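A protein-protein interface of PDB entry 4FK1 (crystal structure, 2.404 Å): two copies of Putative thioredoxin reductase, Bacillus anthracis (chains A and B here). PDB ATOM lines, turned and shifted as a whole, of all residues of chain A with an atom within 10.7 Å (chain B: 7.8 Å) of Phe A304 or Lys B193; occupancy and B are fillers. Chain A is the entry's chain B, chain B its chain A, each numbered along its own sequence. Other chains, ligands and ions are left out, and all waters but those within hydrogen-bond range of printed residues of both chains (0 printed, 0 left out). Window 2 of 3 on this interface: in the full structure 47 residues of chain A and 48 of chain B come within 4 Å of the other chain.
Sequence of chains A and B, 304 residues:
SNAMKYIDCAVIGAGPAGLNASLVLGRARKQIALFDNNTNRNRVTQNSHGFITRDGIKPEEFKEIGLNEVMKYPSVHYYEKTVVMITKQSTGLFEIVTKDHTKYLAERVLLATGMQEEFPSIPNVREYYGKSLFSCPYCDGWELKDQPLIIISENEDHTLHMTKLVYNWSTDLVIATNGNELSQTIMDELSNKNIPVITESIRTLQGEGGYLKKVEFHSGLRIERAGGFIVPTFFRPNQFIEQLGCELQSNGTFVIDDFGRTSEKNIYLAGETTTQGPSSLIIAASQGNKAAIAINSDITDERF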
ATOM      1  N   LYS A  30     -14.937 -33.892 -23.555  1.00  0.00           N
ATOM      2  CA  LYS A  30     -15.194 -34.252 -24.941  1.00  0.00           C
ATOM      3  C   LYS A  30     -16.693 -34.374 -25.181  1.00  0.00           C
ATOM      4  O   LYS A  30     -17.445 -34.723 -24.273  1.00  0.00           O
ATOM      5  CB  LYS A  30     -14.493 -35.568 -25.292  1.00  0.00           C
ATOM      6  CG  LYS A  30     -12.975 -35.477 -25.311  1.00  0.00           C
ATOM      7  CD  LYS A  30     -12.494 -34.522 -26.399  1.00  0.00           C
ATOM      8  CE  LYS A  30     -11.012 -34.196 -26.258  1.00  0.00           C
ATOM      9  NZ  LYS A  30     -10.698 -33.412 -25.018  1.00  0.00           N
ATOM     10  N   GLU A 107     -16.539 -37.333 -35.080  1.00  0.00           N
ATOM     11  CA  GLU A 107     -15.126 -37.422 -35.443  1.00  0.00           C
ATOM     12  C   GLU A 107     -14.556 -38.830 -35.257  1.00  0.00           C
ATOM     13  O   GLU A 107     -13.942 -39.386 -36.172  1.00  0.00           O
ATOM     14  CB  GLU A 107     -14.319 -36.410 -34.619  1.00  0.00           C
ATOM     15  CG  GLU A 107     -12.823 -36.406 -34.889  1.00  0.00           C
ATOM     16  CD  GLU A 107     -12.141 -35.139 -34.392  1.00  0.00           C
ATOM     17  OE1 GLU A 107     -12.641 -34.516 -33.431  1.00  0.00           O
ATOM     18  OE2 GLU A 107     -11.103 -34.760 -34.974  1.00  0.00           O
ATOM     19  N   ARG A 108     -14.759 -39.399 -34.071  1.00  0.00           N
ATOM     20  CA  ARG A 108     -14.250 -40.732 -33.758  1.00  0.00           C
ATOM     21  C   ARG A 108     -15.339 -41.719 -33.315  1.00  0.00           C
ATOM     22  O   ARG A 108     -16.363 -41.331 -32.761  1.00  0.00           O
ATOM     23  CB  ARG A 108     -13.141 -40.643 -32.713  1.00  0.00           C
ATOM     24  CG  ARG A 108     -11.810 -40.232 -33.300  1.00  0.00           C
ATOM     25  CD  ARG A 108     -10.700 -40.245 -32.269  1.00  0.00           C
ATOM     26  NE  ARG A 108      -9.403 -40.013 -32.897  1.00  0.00           N
ATOM     27  CZ  ARG A 108      -8.951 -38.808 -33.237  1.00  0.00           C
ATOM     28  NH1 ARG A 108      -7.762 -38.688 -33.810  1.00  0.00           N
ATOM     29  NH2 ARG A 108      -9.689 -37.725 -33.010  1.00  0.00           N
ATOM     30  N   ASN A 296      -8.780 -39.742 -25.995  1.00  0.00           N
ATOM     31  CA  ASN A 296      -8.334 -38.428 -25.573  1.00  0.00           C
ATOM     32  C   ASN A 296      -6.871 -38.165 -25.936  1.00  0.00           C
ATOM     33  O   ASN A 296      -6.511 -37.052 -26.306  1.00  0.00           O
ATOM     34  CB  ASN A 296      -8.551 -38.245 -24.071  1.00  0.00           C
ATOM     35  CG  ASN A 296      -8.461 -36.787 -23.650  1.00  0.00           C
ATOM     36  OD1 ASN A 296      -7.486 -36.365 -23.030  1.00  0.00           O
ATOM     37  ND2 ASN A 296      -9.478 -36.007 -23.999  1.00  0.00           N
ATOM     38  N   SER A 297      -6.042 -39.201 -25.846  1.00  0.00           N
ATOM     39  CA  SER A 297      -4.618 -39.096 -26.158  1.00  0.00           C
ATOM     40  C   SER A 297      -4.366 -38.849 -27.650  1.00  0.00           C
ATOM     41  O   SER A 297      -3.441 -38.117 -28.023  1.00  0.00           O
ATOM     42  CB  SER A 297      -3.875 -40.352 -25.685  1.00  0.00           C
ATOM     43  OG  SER A 297      -2.483 -40.267 -25.934  1.00  0.00           O
ATOM     44  N   ASP A 298      -5.193 -39.451 -28.498  1.00  0.00           N
ATOM     45  CA  ASP A 298      -5.091 -39.249 -29.943  1.00  0.00           C
ATOM     46  C   ASP A 298      -5.673 -37.915 -30.424  1.00  0.00           C
ATOM     47  O   ASP A 298      -5.275 -37.390 -31.463  1.00  0.00           O
ATOM     48  CB  ASP A 298      -5.770 -40.395 -30.688  1.00  0.00           C
ATOM     49  CG  ASP A 298      -4.952 -41.662 -30.668  1.00  0.00           C
ATOM     50  OD1 ASP A 298      -3.706 -41.567 -30.700  1.00  0.00           O
ATOM     51  OD2 ASP A 298      -5.557 -42.753 -30.625  1.00  0.00           O
ATOM     52  N   ILE A 299      -6.648 -37.401 -29.684  1.00  0.00           N
ATOM     53  CA  ILE A 299      -7.238 -36.104 -29.968  1.00  0.00           C
ATOM     54  C   ILE A 299      -6.245 -34.995 -29.588  1.00  0.00           C
ATOM     55  O   ILE A 299      -5.873 -34.168 -30.413  1.00  0.00           O
ATOM     56  CB  ILE A 299      -8.555 -35.917 -29.194  1.00  0.00           C
ATOM     57  CG1 ILE A 299      -9.647 -36.812 -29.771  1.00  0.00           C
ATOM     58  CG2 ILE A 299      -9.013 -34.475 -29.267  1.00  0.00           C
ATOM     59  CD1 ILE A 299     -10.985 -36.594 -29.123  1.00  0.00           C
ATOM     60  N   THR A 300      -5.811 -35.013 -28.333  1.00  0.00           N
ATOM     61  CA  THR A 300      -4.782 -34.116 -27.826  1.00  0.00           C
ATOM     62  C   THR A 300      -3.568 -34.036 -28.747  1.00  0.00           C
ATOM     63  O   THR A 300      -3.023 -32.960 -28.977  1.00  0.00           O
ATOM     64  CB  THR A 300      -4.334 -34.574 -26.425  1.00  0.00           C
ATOM     65  OG1 THR A 300      -5.304 -34.157 -25.458  1.00  0.00           O
ATOM     66  CG2 THR A 300      -2.981 -33.994 -26.064  1.00  0.00           C
ATOM     67  N   ASP A 301      -3.156 -35.177 -29.285  1.00  0.00           N
ATOM     68  CA  ASP A 301      -2.010 -35.229 -30.183  1.00  0.00           C
ATOM     69  C   ASP A 301      -2.237 -34.352 -31.409  1.00  0.00           C
ATOM     70  O   ASP A 301      -1.350 -33.594 -31.817  1.00  0.00           O
ATOM     71  CB  ASP A 301      -1.725 -36.672 -30.613  1.00  0.00           C
ATOM     72  CG  ASP A 301      -0.398 -37.192 -30.081  1.00  0.00           C
ATOM     73  OD1 ASP A 301      -0.392 -38.247 -29.404  1.00  0.00           O
ATOM     74  OD2 ASP A 301       0.641 -36.551 -30.348  1.00  0.00           O
ATOM     75  N   GLU A 302      -3.438 -34.445 -31.976  1.00  0.00           N
ATOM     76  CA  GLU A 302      -3.763 -33.749 -33.220  1.00  0.00           C
ATOM     77  C   GLU A 302      -4.176 -32.290 -33.011  1.00  0.00           C
ATOM     78  O   GLU A 302      -3.978 -31.458 -33.893  1.00  0.00           O
ATOM     79  CB  GLU A 302      -4.845 -34.512 -34.008  1.00  0.00           C
ATOM     80  CG  GLU A 302      -6.286 -34.181 -33.615  1.00  0.00           C
ATOM     81  CD  GLU A 302      -7.310 -35.160 -34.185  1.00  0.00           C
ATOM     82  OE1 GLU A 302      -6.907 -36.222 -34.708  1.00  0.00           O
ATOM     83  OE2 GLU A 302      -8.523 -34.863 -34.104  1.00  0.00           O
ATOM     84  N   ARG A 303      -4.744 -31.986 -31.848  1.00  0.00           N
ATOM     85  CA  ARG A 303      -5.272 -30.649 -31.578  1.00  0.00           C
ATOM     86  C   ARG A 303      -4.193 -29.674 -31.075  1.00  0.00           C
ATOM     87  O   ARG A 303      -4.285 -28.465 -31.299  1.00  0.00           O
ATOM     88  CB  ARG A 303      -6.433 -30.715 -30.580  1.00  0.00           C
ATOM     89  CG  ARG A 303      -7.499 -31.720 -30.953  1.00  0.00           C
ATOM     90  CD  ARG A 303      -8.653 -31.087 -31.697  1.00  0.00           C
ATOM     91  NE  ARG A 303      -9.862 -30.979 -30.881  1.00  0.00           N
ATOM     92  CZ  ARG A 303     -10.865 -31.854 -30.910  1.00  0.00           C
ATOM     93  NH1 ARG A 303     -10.791 -32.920 -31.708  1.00  0.00           N
ATOM     94  NH2 ARG A 303     -11.934 -31.666 -30.139  1.00  0.00           N
ATOM     95  N   PHE A 304      -3.172 -30.204 -30.404  1.00  0.00           N
ATOM     96  CA  PHE A 304      -2.088 -29.365 -29.891  1.00  0.00           C
ATOM     97  C   PHE A 304      -1.298 -28.696 -31.032  1.00  0.00           C
ATOM     98  O   PHE A 304      -1.023 -27.492 -30.991  1.00  0.00           O
ATOM     99  CB  PHE A 304      -1.153 -30.173 -28.977  1.00  0.00           C
ATOM    100  CG  PHE A 304      -0.544 -29.363 -27.862  1.00  0.00           C
ATOM    101  CD1 PHE A 304      -1.356 -28.706 -26.938  1.00  0.00           C
ATOM    102  CD2 PHE A 304       0.832 -29.262 -27.738  1.00  0.00           C
ATOM    103  CE1 PHE A 304      -0.798 -27.960 -25.913  1.00  0.00           C
ATOM    104  CE2 PHE A 304       1.396 -28.530 -26.724  1.00  0.00           C
ATOM    105  CZ  PHE A 304       0.588 -27.873 -25.806  1.00  0.00           C
ATOM    106  N   LEU B 160       6.519 -32.463 -21.618  1.00  0.00           N
ATOM    107  CA  LEU B 160       5.815 -32.182 -22.860  1.00  0.00           C
ATOM    108  C   LEU B 160       4.474 -32.915 -22.925  1.00  0.00           C
ATOM    109  O   LEU B 160       3.428 -32.301 -23.148  1.00  0.00           O
ATOM    110  CB  LEU B 160       6.691 -32.542 -24.057  1.00  0.00           C
ATOM    111  CG  LEU B 160       6.077 -32.257 -25.425  1.00  0.00           C
ATOM    112  CD1 LEU B 160       5.551 -30.825 -25.491  1.00  0.00           C
ATOM    113  CD2 LEU B 160       7.102 -32.511 -26.513  1.00  0.00           C
ATOM    114  N   HIS B 161       4.516 -34.224 -22.712  1.00  0.00           N
ATOM    115  CA  HIS B 161       3.309 -35.042 -22.698  1.00  0.00           C
ATOM    116  C   HIS B 161       2.325 -34.591 -21.622  1.00  0.00           C
ATOM    117  O   HIS B 161       1.156 -34.329 -21.899  1.00  0.00           O
ATOM    118  CB  HIS B 161       3.677 -36.514 -22.481  1.00  0.00           C
ATOM    119  CG  HIS B 161       2.496 -37.413 -22.281  1.00  0.00           C
ATOM    120  ND1 HIS B 161       1.854 -37.541 -21.066  1.00  0.00           N
ATOM    121  CD2 HIS B 161       1.849 -38.241 -23.136  1.00  0.00           C
ATOM    122  CE1 HIS B 161       0.862 -38.403 -21.182  1.00  0.00           C
ATOM    123  NE2 HIS B 161       0.838 -38.847 -22.427  1.00  0.00           N
ATOM    124  N   THR B 163       2.021 -31.788 -20.153  1.00  0.00           N
ATOM    125  CA  THR B 163       1.409 -30.510 -20.494  1.00  0.00           C
ATOM    126  C   THR B 163       0.255 -30.662 -21.483  1.00  0.00           C
ATOM    127  O   THR B 163      -0.852 -30.212 -21.204  1.00  0.00           O
ATOM    128  CB  THR B 163       2.435 -29.505 -21.044  1.00  0.00           C
ATOM    129  OG1 THR B 163       3.442 -29.266 -20.056  1.00  0.00           O
ATOM    130  CG2 THR B 163       1.750 -28.196 -21.374  1.00  0.00           C
ATOM    131  N   LYS B 164       0.518 -31.310 -22.618  1.00  0.00           N
ATOM    132  CA  LYS B 164      -0.483 -31.465 -23.676  1.00  0.00           C
ATOM    133  C   LYS B 164      -1.771 -32.055 -23.112  1.00  0.00           C
ATOM    134  O   LYS B 164      -2.874 -31.621 -23.451  1.00  0.00           O
ATOM    135  CB  LYS B 164       0.030 -32.364 -24.803  1.00  0.00           C
ATOM    136  CG  LYS B 164       1.290 -31.907 -25.497  1.00  0.00           C
ATOM    137  CD  LYS B 164       1.429 -32.600 -26.840  1.00  0.00           C
ATOM    138  CE  LYS B 164       2.701 -32.195 -27.557  1.00  0.00           C
ATOM    139  NZ  LYS B 164       2.597 -32.457 -29.024  1.00  0.00           N
ATOM    140  N   LEU B 165      -1.609 -33.035 -22.230  1.00  0.00           N
ATOM    141  CA  LEU B 165      -2.726 -33.686 -21.558  1.00  0.00           C
ATOM    142  C   LEU B 165      -3.458 -32.750 -20.592  1.00  0.00           C
ATOM    143  O   LEU B 165      -4.678 -32.666 -20.614  1.00  0.00           O
ATOM    144  CB  LEU B 165      -2.216 -34.921 -20.818  1.00  0.00           C
ATOM    145  CG  LEU B 165      -3.219 -35.767 -20.038  1.00  0.00           C
ATOM    146  CD1 LEU B 165      -4.434 -36.086 -20.875  1.00  0.00           C
ATOM    147  CD2 LEU B 165      -2.543 -37.053 -19.559  1.00  0.00           C
ATOM    148  N   VAL B 166      -2.707 -32.062 -19.739  1.00  0.00           N
ATOM    149  CA  VAL B 166      -3.292 -31.156 -18.758  1.00  0.00           C
ATOM    150  C   VAL B 166      -4.077 -30.036 -19.435  1.00  0.00           C
ATOM    151  O   VAL B 166      -5.146 -29.646 -18.970  1.00  0.00           O
ATOM    152  CB  VAL B 166      -2.215 -30.561 -17.834  1.00  0.00           C
ATOM    153  CG1 VAL B 166      -2.739 -29.328 -17.138  1.00  0.00           C
ATOM    154  CG2 VAL B 166      -1.796 -31.594 -16.807  1.00  0.00           C
ATOM    155  N   TYR B 167      -3.547 -29.554 -20.554  1.00  0.00           N
ATOM    156  CA  TYR B 167      -4.176 -28.509 -21.355  1.00  0.00           C
ATOM    157  C   TYR B 167      -5.635 -28.825 -21.748  1.00  0.00           C
ATOM    158  O   TYR B 167      -6.386 -27.924 -22.131  1.00  0.00           O
ATOM    159  CB  TYR B 167      -3.312 -28.249 -22.599  1.00  0.00           C
ATOM    160  CG  TYR B 167      -3.648 -27.004 -23.400  1.00  0.00           C
ATOM    161  CD1 TYR B 167      -4.455 -27.082 -24.528  1.00  0.00           C
ATOM    162  CD2 TYR B 167      -3.135 -25.752 -23.045  1.00  0.00           C
ATOM    163  CE1 TYR B 167      -4.752 -25.957 -25.274  1.00  0.00           C
ATOM    164  CE2 TYR B 167      -3.438 -24.614 -23.792  1.00  0.00           C
ATOM    165  CZ  TYR B 167      -4.243 -24.729 -24.905  1.00  0.00           C
ATOM    166  OH  TYR B 167      -4.555 -23.624 -25.663  1.00  0.00           O
ATOM    167  N   ASN B 168      -6.034 -30.093 -21.650  1.00  0.00           N
ATOM    168  CA  ASN B 168      -7.432 -30.469 -21.873  1.00  0.00           C
ATOM    169  C   ASN B 168      -8.392 -29.796 -20.893  1.00  0.00           C
ATOM    170  O   ASN B 168      -9.536 -29.478 -21.236  1.00  0.00           O
ATOM    171  CB  ASN B 168      -7.648 -31.998 -21.754  1.00  0.00           C
ATOM    172  CG  ASN B 168      -7.393 -32.748 -23.053  1.00  0.00           C
ATOM    173  OD1 ASN B 168      -8.189 -32.687 -23.984  1.00  0.00           O
ATOM    174  ND2 ASN B 168      -6.284 -33.483 -23.105  1.00  0.00           N
ATOM    175  N   THR B 171      -6.414 -24.055 -20.192  1.00  0.00           N
ATOM    176  CA  THR B 171      -5.459 -23.461 -21.118  1.00  0.00           C
ATOM    177  C   THR B 171      -4.577 -22.427 -20.413  1.00  0.00           C
ATOM    178  O   THR B 171      -3.737 -21.784 -21.042  1.00  0.00           O
ATOM    179  CB  THR B 171      -6.174 -22.788 -22.296  1.00  0.00           C
ATOM    180  OG1 THR B 171      -7.118 -21.836 -21.796  1.00  0.00           O
ATOM    181  CG2 THR B 171      -6.922 -23.806 -23.112  1.00  0.00           C
ATOM    182  N   ASP B 172      -4.768 -22.271 -19.107  1.00  0.00           N
ATOM    183  CA  ASP B 172      -3.978 -21.323 -18.328  1.00  0.00           C
ATOM    184  C   ASP B 172      -2.925 -22.052 -17.495  1.00  0.00           C
ATOM    185  O   ASP B 172      -3.151 -22.348 -16.326  1.00  0.00           O
ATOM    186  CB  ASP B 172      -4.887 -20.490 -17.422  1.00  0.00           C
ATOM    187  CG  ASP B 172      -4.121 -19.434 -16.631  1.00  0.00           C
ATOM    188  OD1 ASP B 172      -2.981 -19.083 -17.019  1.00  0.00           O
ATOM    189  OD2 ASP B 172      -4.667 -18.951 -15.618  1.00  0.00           O
ATOM    190  N   LEU B 173      -1.767 -22.322 -18.095  1.00  0.00           N
ATOM    191  CA  LEU B 173      -0.751 -23.167 -17.475  1.00  0.00           C
ATOM    192  C   LEU B 173       0.617 -22.478 -17.309  1.00  0.00           C
ATOM    193  O   LEU B 173       1.061 -21.721 -18.175  1.00  0.00           O
ATOM    194  CB  LEU B 173      -0.580 -24.452 -18.294  1.00  0.00           C
ATOM    195  CG  LEU B 173      -1.818 -25.336 -18.437  1.00  0.00           C
ATOM    196  CD1 LEU B 173      -1.523 -26.614 -19.245  1.00  0.00           C
ATOM    197  CD2 LEU B 173      -2.374 -25.677 -17.060  1.00  0.00           C
ATOM    198  N   ILE B 186      11.117 -27.855 -26.470  1.00  0.00           N
ATOM    199  CA  ILE B 186       9.923 -27.891 -25.636  1.00  0.00           C
ATOM    200  C   ILE B 186       9.513 -26.484 -25.195  1.00  0.00           C
ATOM    201  O   ILE B 186       8.332 -26.150 -25.159  1.00  0.00           O
ATOM    202  CB  ILE B 186      10.081 -28.849 -24.427  1.00  0.00           C
ATOM    203  CG1 ILE B 186      10.421 -30.264 -24.910  1.00  0.00           C
ATOM    204  CG2 ILE B 186       8.810 -28.867 -23.586  1.00  0.00           C
ATOM    205  CD1 ILE B 186      10.156 -31.346 -23.886  1.00  0.00           C
ATOM    206  N   MET B 187      10.499 -25.653 -24.895  1.00  0.00           N
ATOM    207  CA  MET B 187      10.225 -24.280 -24.484  1.00  0.00           C
ATOM    208  C   MET B 187       9.449 -23.489 -25.541  1.00  0.00           C
ATOM    209  O   MET B 187       8.481 -22.794 -25.219  1.00  0.00           O
ATOM    210  CB  MET B 187      11.523 -23.562 -24.141  1.00  0.00           C
ATOM    211  CG  MET B 187      12.315 -24.188 -23.007  1.00  0.00           C
ATOM    212  SD  MET B 187      13.567 -22.956 -22.173  1.00  0.00           S
ATOM    213  CE  MET B 187      14.206 -21.961 -23.748  1.00  0.00           C
ATOM    214  N   ASP B 188       9.874 -23.610 -26.798  1.00  0.00           N
ATOM    215  CA  ASP B 188       9.251 -22.876 -27.898  1.00  0.00           C
ATOM    216  C   ASP B 188       7.852 -23.381 -28.241  1.00  0.00           C
ATOM    217  O   ASP B 188       6.972 -22.601 -28.616  1.00  0.00           O
ATOM    218  CB  ASP B 188      10.139 -22.912 -29.144  1.00  0.00           C
ATOM    219  CG  ASP B 188      11.075 -21.720 -29.228  1.00  0.00           C
ATOM    220  OD1 ASP B 188      10.803 -20.703 -28.551  1.00  0.00           O
ATOM    221  OD2 ASP B 188      12.074 -21.800 -29.977  1.00  0.00           O
ATOM    222  N   GLU B 189       7.656 -24.688 -28.129  1.00  0.00           N
ATOM    223  CA  GLU B 189       6.363 -25.274 -28.432  1.00  0.00           C
ATOM    224  C   GLU B 189       5.327 -24.884 -27.391  1.00  0.00           C
ATOM    225  O   GLU B 189       4.203 -24.520 -27.734  1.00  0.00           O
ATOM    226  CB  GLU B 189       6.478 -26.788 -28.552  1.00  0.00           C
ATOM    227  CG  GLU B 189       7.265 -27.216 -29.771  1.00  0.00           C
ATOM    228  CD  GLU B 189       7.339 -28.717 -29.903  1.00  0.00           C
ATOM    229  OE1 GLU B 189       6.934 -29.412 -28.944  1.00  0.00           O
ATOM    230  OE2 GLU B 189       7.799 -29.194 -30.966  1.00  0.00           O
ATOM    231  N   LEU B 190       5.704 -24.944 -26.119  1.00  0.00           N
ATOM    232  CA  LEU B 190       4.806 -24.496 -25.061  1.00  0.00           C
ATOM    233  C   LEU B 190       4.527 -22.994 -25.157  1.00  0.00           C
ATOM    234  O   LEU B 190       3.367 -22.575 -25.137  1.00  0.00           O
ATOM    235  CB  LEU B 190       5.347 -24.858 -23.669  1.00  0.00           C
ATOM    236  CG  LEU B 190       4.865 -26.180 -23.055  1.00  0.00           C
ATOM    237  CD1 LEU B 190       5.328 -27.365 -23.892  1.00  0.00           C
ATOM    238  CD2 LEU B 190       5.356 -26.302 -21.621  1.00  0.00           C
ATOM    239  N   SER B 191       5.586 -22.191 -25.276  1.00  0.00           N
ATOM    240  CA  SER B 191       5.454 -20.734 -25.330  1.00  0.00           C
ATOM    241  C   SER B 191       4.643 -20.279 -26.534  1.00  0.00           C
ATOM    242  O   SER B 191       4.080 -19.189 -26.535  1.00  0.00           O
ATOM    243  CB  SER B 191       6.828 -20.068 -25.336  1.00  0.00           C
ATOM    244  OG  SER B 191       7.014 -19.287 -26.504  1.00  0.00           O
ATOM    245  N   ASN B 192       4.583 -21.131 -27.553  1.00  0.00           N
ATOM    246  CA  ASN B 192       3.761 -20.887 -28.729  1.00  0.00           C
ATOM    247  C   ASN B 192       2.280 -21.108 -28.422  1.00  0.00           C
ATOM    248  O   ASN B 192       1.412 -20.805 -29.247  1.00  0.00           O
ATOM    249  CB  ASN B 192       4.213 -21.795 -29.874  1.00  0.00           C
ATOM    250  CG  ASN B 192       3.909 -21.217 -31.239  1.00  0.00           C
ATOM    251  OD1 ASN B 192       4.458 -20.179 -31.625  1.00  0.00           O
ATOM    252  ND2 ASN B 192       3.045 -21.896 -31.991  1.00  0.00           N
ATOM    253  N   LYS B 193       2.006 -21.648 -27.234  1.00  0.00           N
ATOM    254  CA  LYS B 193       0.641 -21.875 -26.754  1.00  0.00           C
ATOM    255  C   LYS B 193       0.312 -20.945 -25.587  1.00  0.00           C
ATOM    256  O   LYS B 193      -0.637 -21.197 -24.833  1.00  0.00           O
ATOM    257  CB  LYS B 193       0.454 -23.331 -26.294  1.00  0.00           C
ATOM    258  CG  LYS B 193       0.509 -24.370 -27.398  1.00  0.00           C
ATOM    259  CD  LYS B 193      -0.643 -24.213 -28.365  1.00  0.00           C
ATOM    260  CE  LYS B 193      -0.258 -24.738 -29.730  1.00  0.00           C
ATOM    261  NZ  LYS B 193      -1.319 -24.496 -30.745  1.00  0.00           N
ATOM    262  N   ASN B 194       1.110 -19.888 -25.437  1.00  0.00           N
ATOM    263  CA  ASN B 194       0.939 -18.917 -24.357  1.00  0.00           C
ATOM    264  C   ASN B 194       1.130 -19.565 -22.990  1.00  0.00           C
ATOM    265  O   ASN B 194       0.540 -19.130 -21.991  1.00  0.00           O
ATOM    266  CB  ASN B 194      -0.426 -18.222 -24.455  1.00  0.00           C
ATOM    267  CG  ASN B 194      -0.409 -16.808 -23.913  1.00  0.00           C
ATOM    268  OD1 ASN B 194      -0.869 -16.558 -22.795  1.00  0.00           O
ATOM    269  ND2 ASN B 194       0.111 -15.868 -24.708  1.00  0.00           N
ATOM    270  N   ILE B 195       1.965 -20.603 -22.963  1.00  0.00           N
ATOM    271  CA  ILE B 195       2.323 -21.313 -21.740  1.00  0.00           C
ATOM    272  C   ILE B 195       3.771 -21.014 -21.380  1.00  0.00           C
ATOM    273  O   ILE B 195       4.688 -21.444 -22.076  1.00  0.00           O
ATOM    274  CB  ILE B 195       2.173 -22.855 -21.914  1.00  0.00           C
ATOM    275  CG1 ILE B 195       0.742 -23.231 -22.298  1.00  0.00           C
ATOM    276  CG2 ILE B 195       2.610 -23.603 -20.657  1.00  0.00           C
ATOM    277  CD1 ILE B 195       0.631 -24.622 -22.857  1.00  0.00           C
ATOM    278  N   PRO B 196       3.982 -20.273 -20.284  1.00  0.00           N
ATOM    279  CA  PRO B 196       5.337 -19.923 -19.832  1.00  0.00           C
ATOM    280  C   PRO B 196       6.028 -21.072 -19.087  1.00  0.00           C
ATOM    281  O   PRO B 196       5.367 -21.993 -18.615  1.00  0.00           O
ATOM    282  CB  PRO B 196       5.090 -18.744 -18.892  1.00  0.00           C
ATOM    283  CG  PRO B 196       3.721 -19.001 -18.342  1.00  0.00           C
ATOM    284  CD  PRO B 196       2.940 -19.627 -19.467  1.00  0.00           C
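O of Phe A304 is in hydrogen-bond range of NZ of Lys B193 (3.0 Å).
The side-chain amino group of Lys A30 lies within hydrogen-bond range of the side-chain amide oxygen of Asn B168, 2.8 Å away.
ND2 of Asn B168 is in hydrogen-bond range of OG1 of Thr A300 (2.6 Å).
The side-chain amide nitrogen (ND2) of Asn B168 lies within hydrogen-bond range of the side-chain amide oxygen (OD1) of Asn A296.
O of Leu B165 lies within hydrogen-bond range of ND2 of Asn B168, 3.1 Å away.
O of Asn A296 is in hydrogen-bond range of OG1 of Thr A300, at 3.2 Å.
ND2 of Asn A296 sits close to NZ of Lys A30, at 3.0 Å.
Among the printed residues, pairs that only touch across the chains: Asn A296 with Leu B165 (3.7 Å), Thr A300 with Lys B164 (3.5 Å), Phe A304 with Lys B164 (3.5 Å) and Phe A304 with Tyr B167 (3.9 Å).
Printed residues of chain B within 4 Å of Asn A296: Leu B165 (3.7 Å) and Asn B168 (3.1 Å).
Of the printed residues of chain B, Thr A300 touches Lys B164 and Asn B168.
Of the printed residues of chain B, Phe A304 touches Lys B164 (3.5 Å), Tyr B167 (3.9 Å) and Lys B193 (3.0 Å).
Lys B164 touches just these residues of chain A: Thr A300 and Phe A304.
Of the printed residues of chain A, Tyr B167 touches Phe A304 (3.9 Å).
Of the printed residues of chain A, Asn B168 touches Lys A30 (2.8 Å), Asn A296 (3.1 Å) and Thr A300 (2.6 Å).
No residue of chain A comes within 4 Å of Ser B191.
Of chain A, only Phe A304 comes within 4 Å of Lys B193.
Asn B194 touches none of the printed residues of chain A.
The nearest residue of chain B that does not touch Phe A304 is Ile B195 (4.4 Å).
The nearest residue of chain A that does not touch Lys B193 is Arg A303 (5.0 Å).
The nearest printed residue of chain B that does not touch Lys A30 is Leu B165 (7.5 Å).
Hydrophobic or aromatic side chains of chain A that line the printed part of chain B: Phe A304.
Printed residues of chain B that touch a printed residue of chain A: Lys B164, Leu B165, Tyr B167, Asn B168 and Lys B193.
Among the printed residues, 8 pairs touch across the chains.
Among the printed residues, no Asp or Glu carboxylate lies within 4 Å of a Lys or Arg side-chain nitrogen of the other chain.
No position is printed for both chains.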
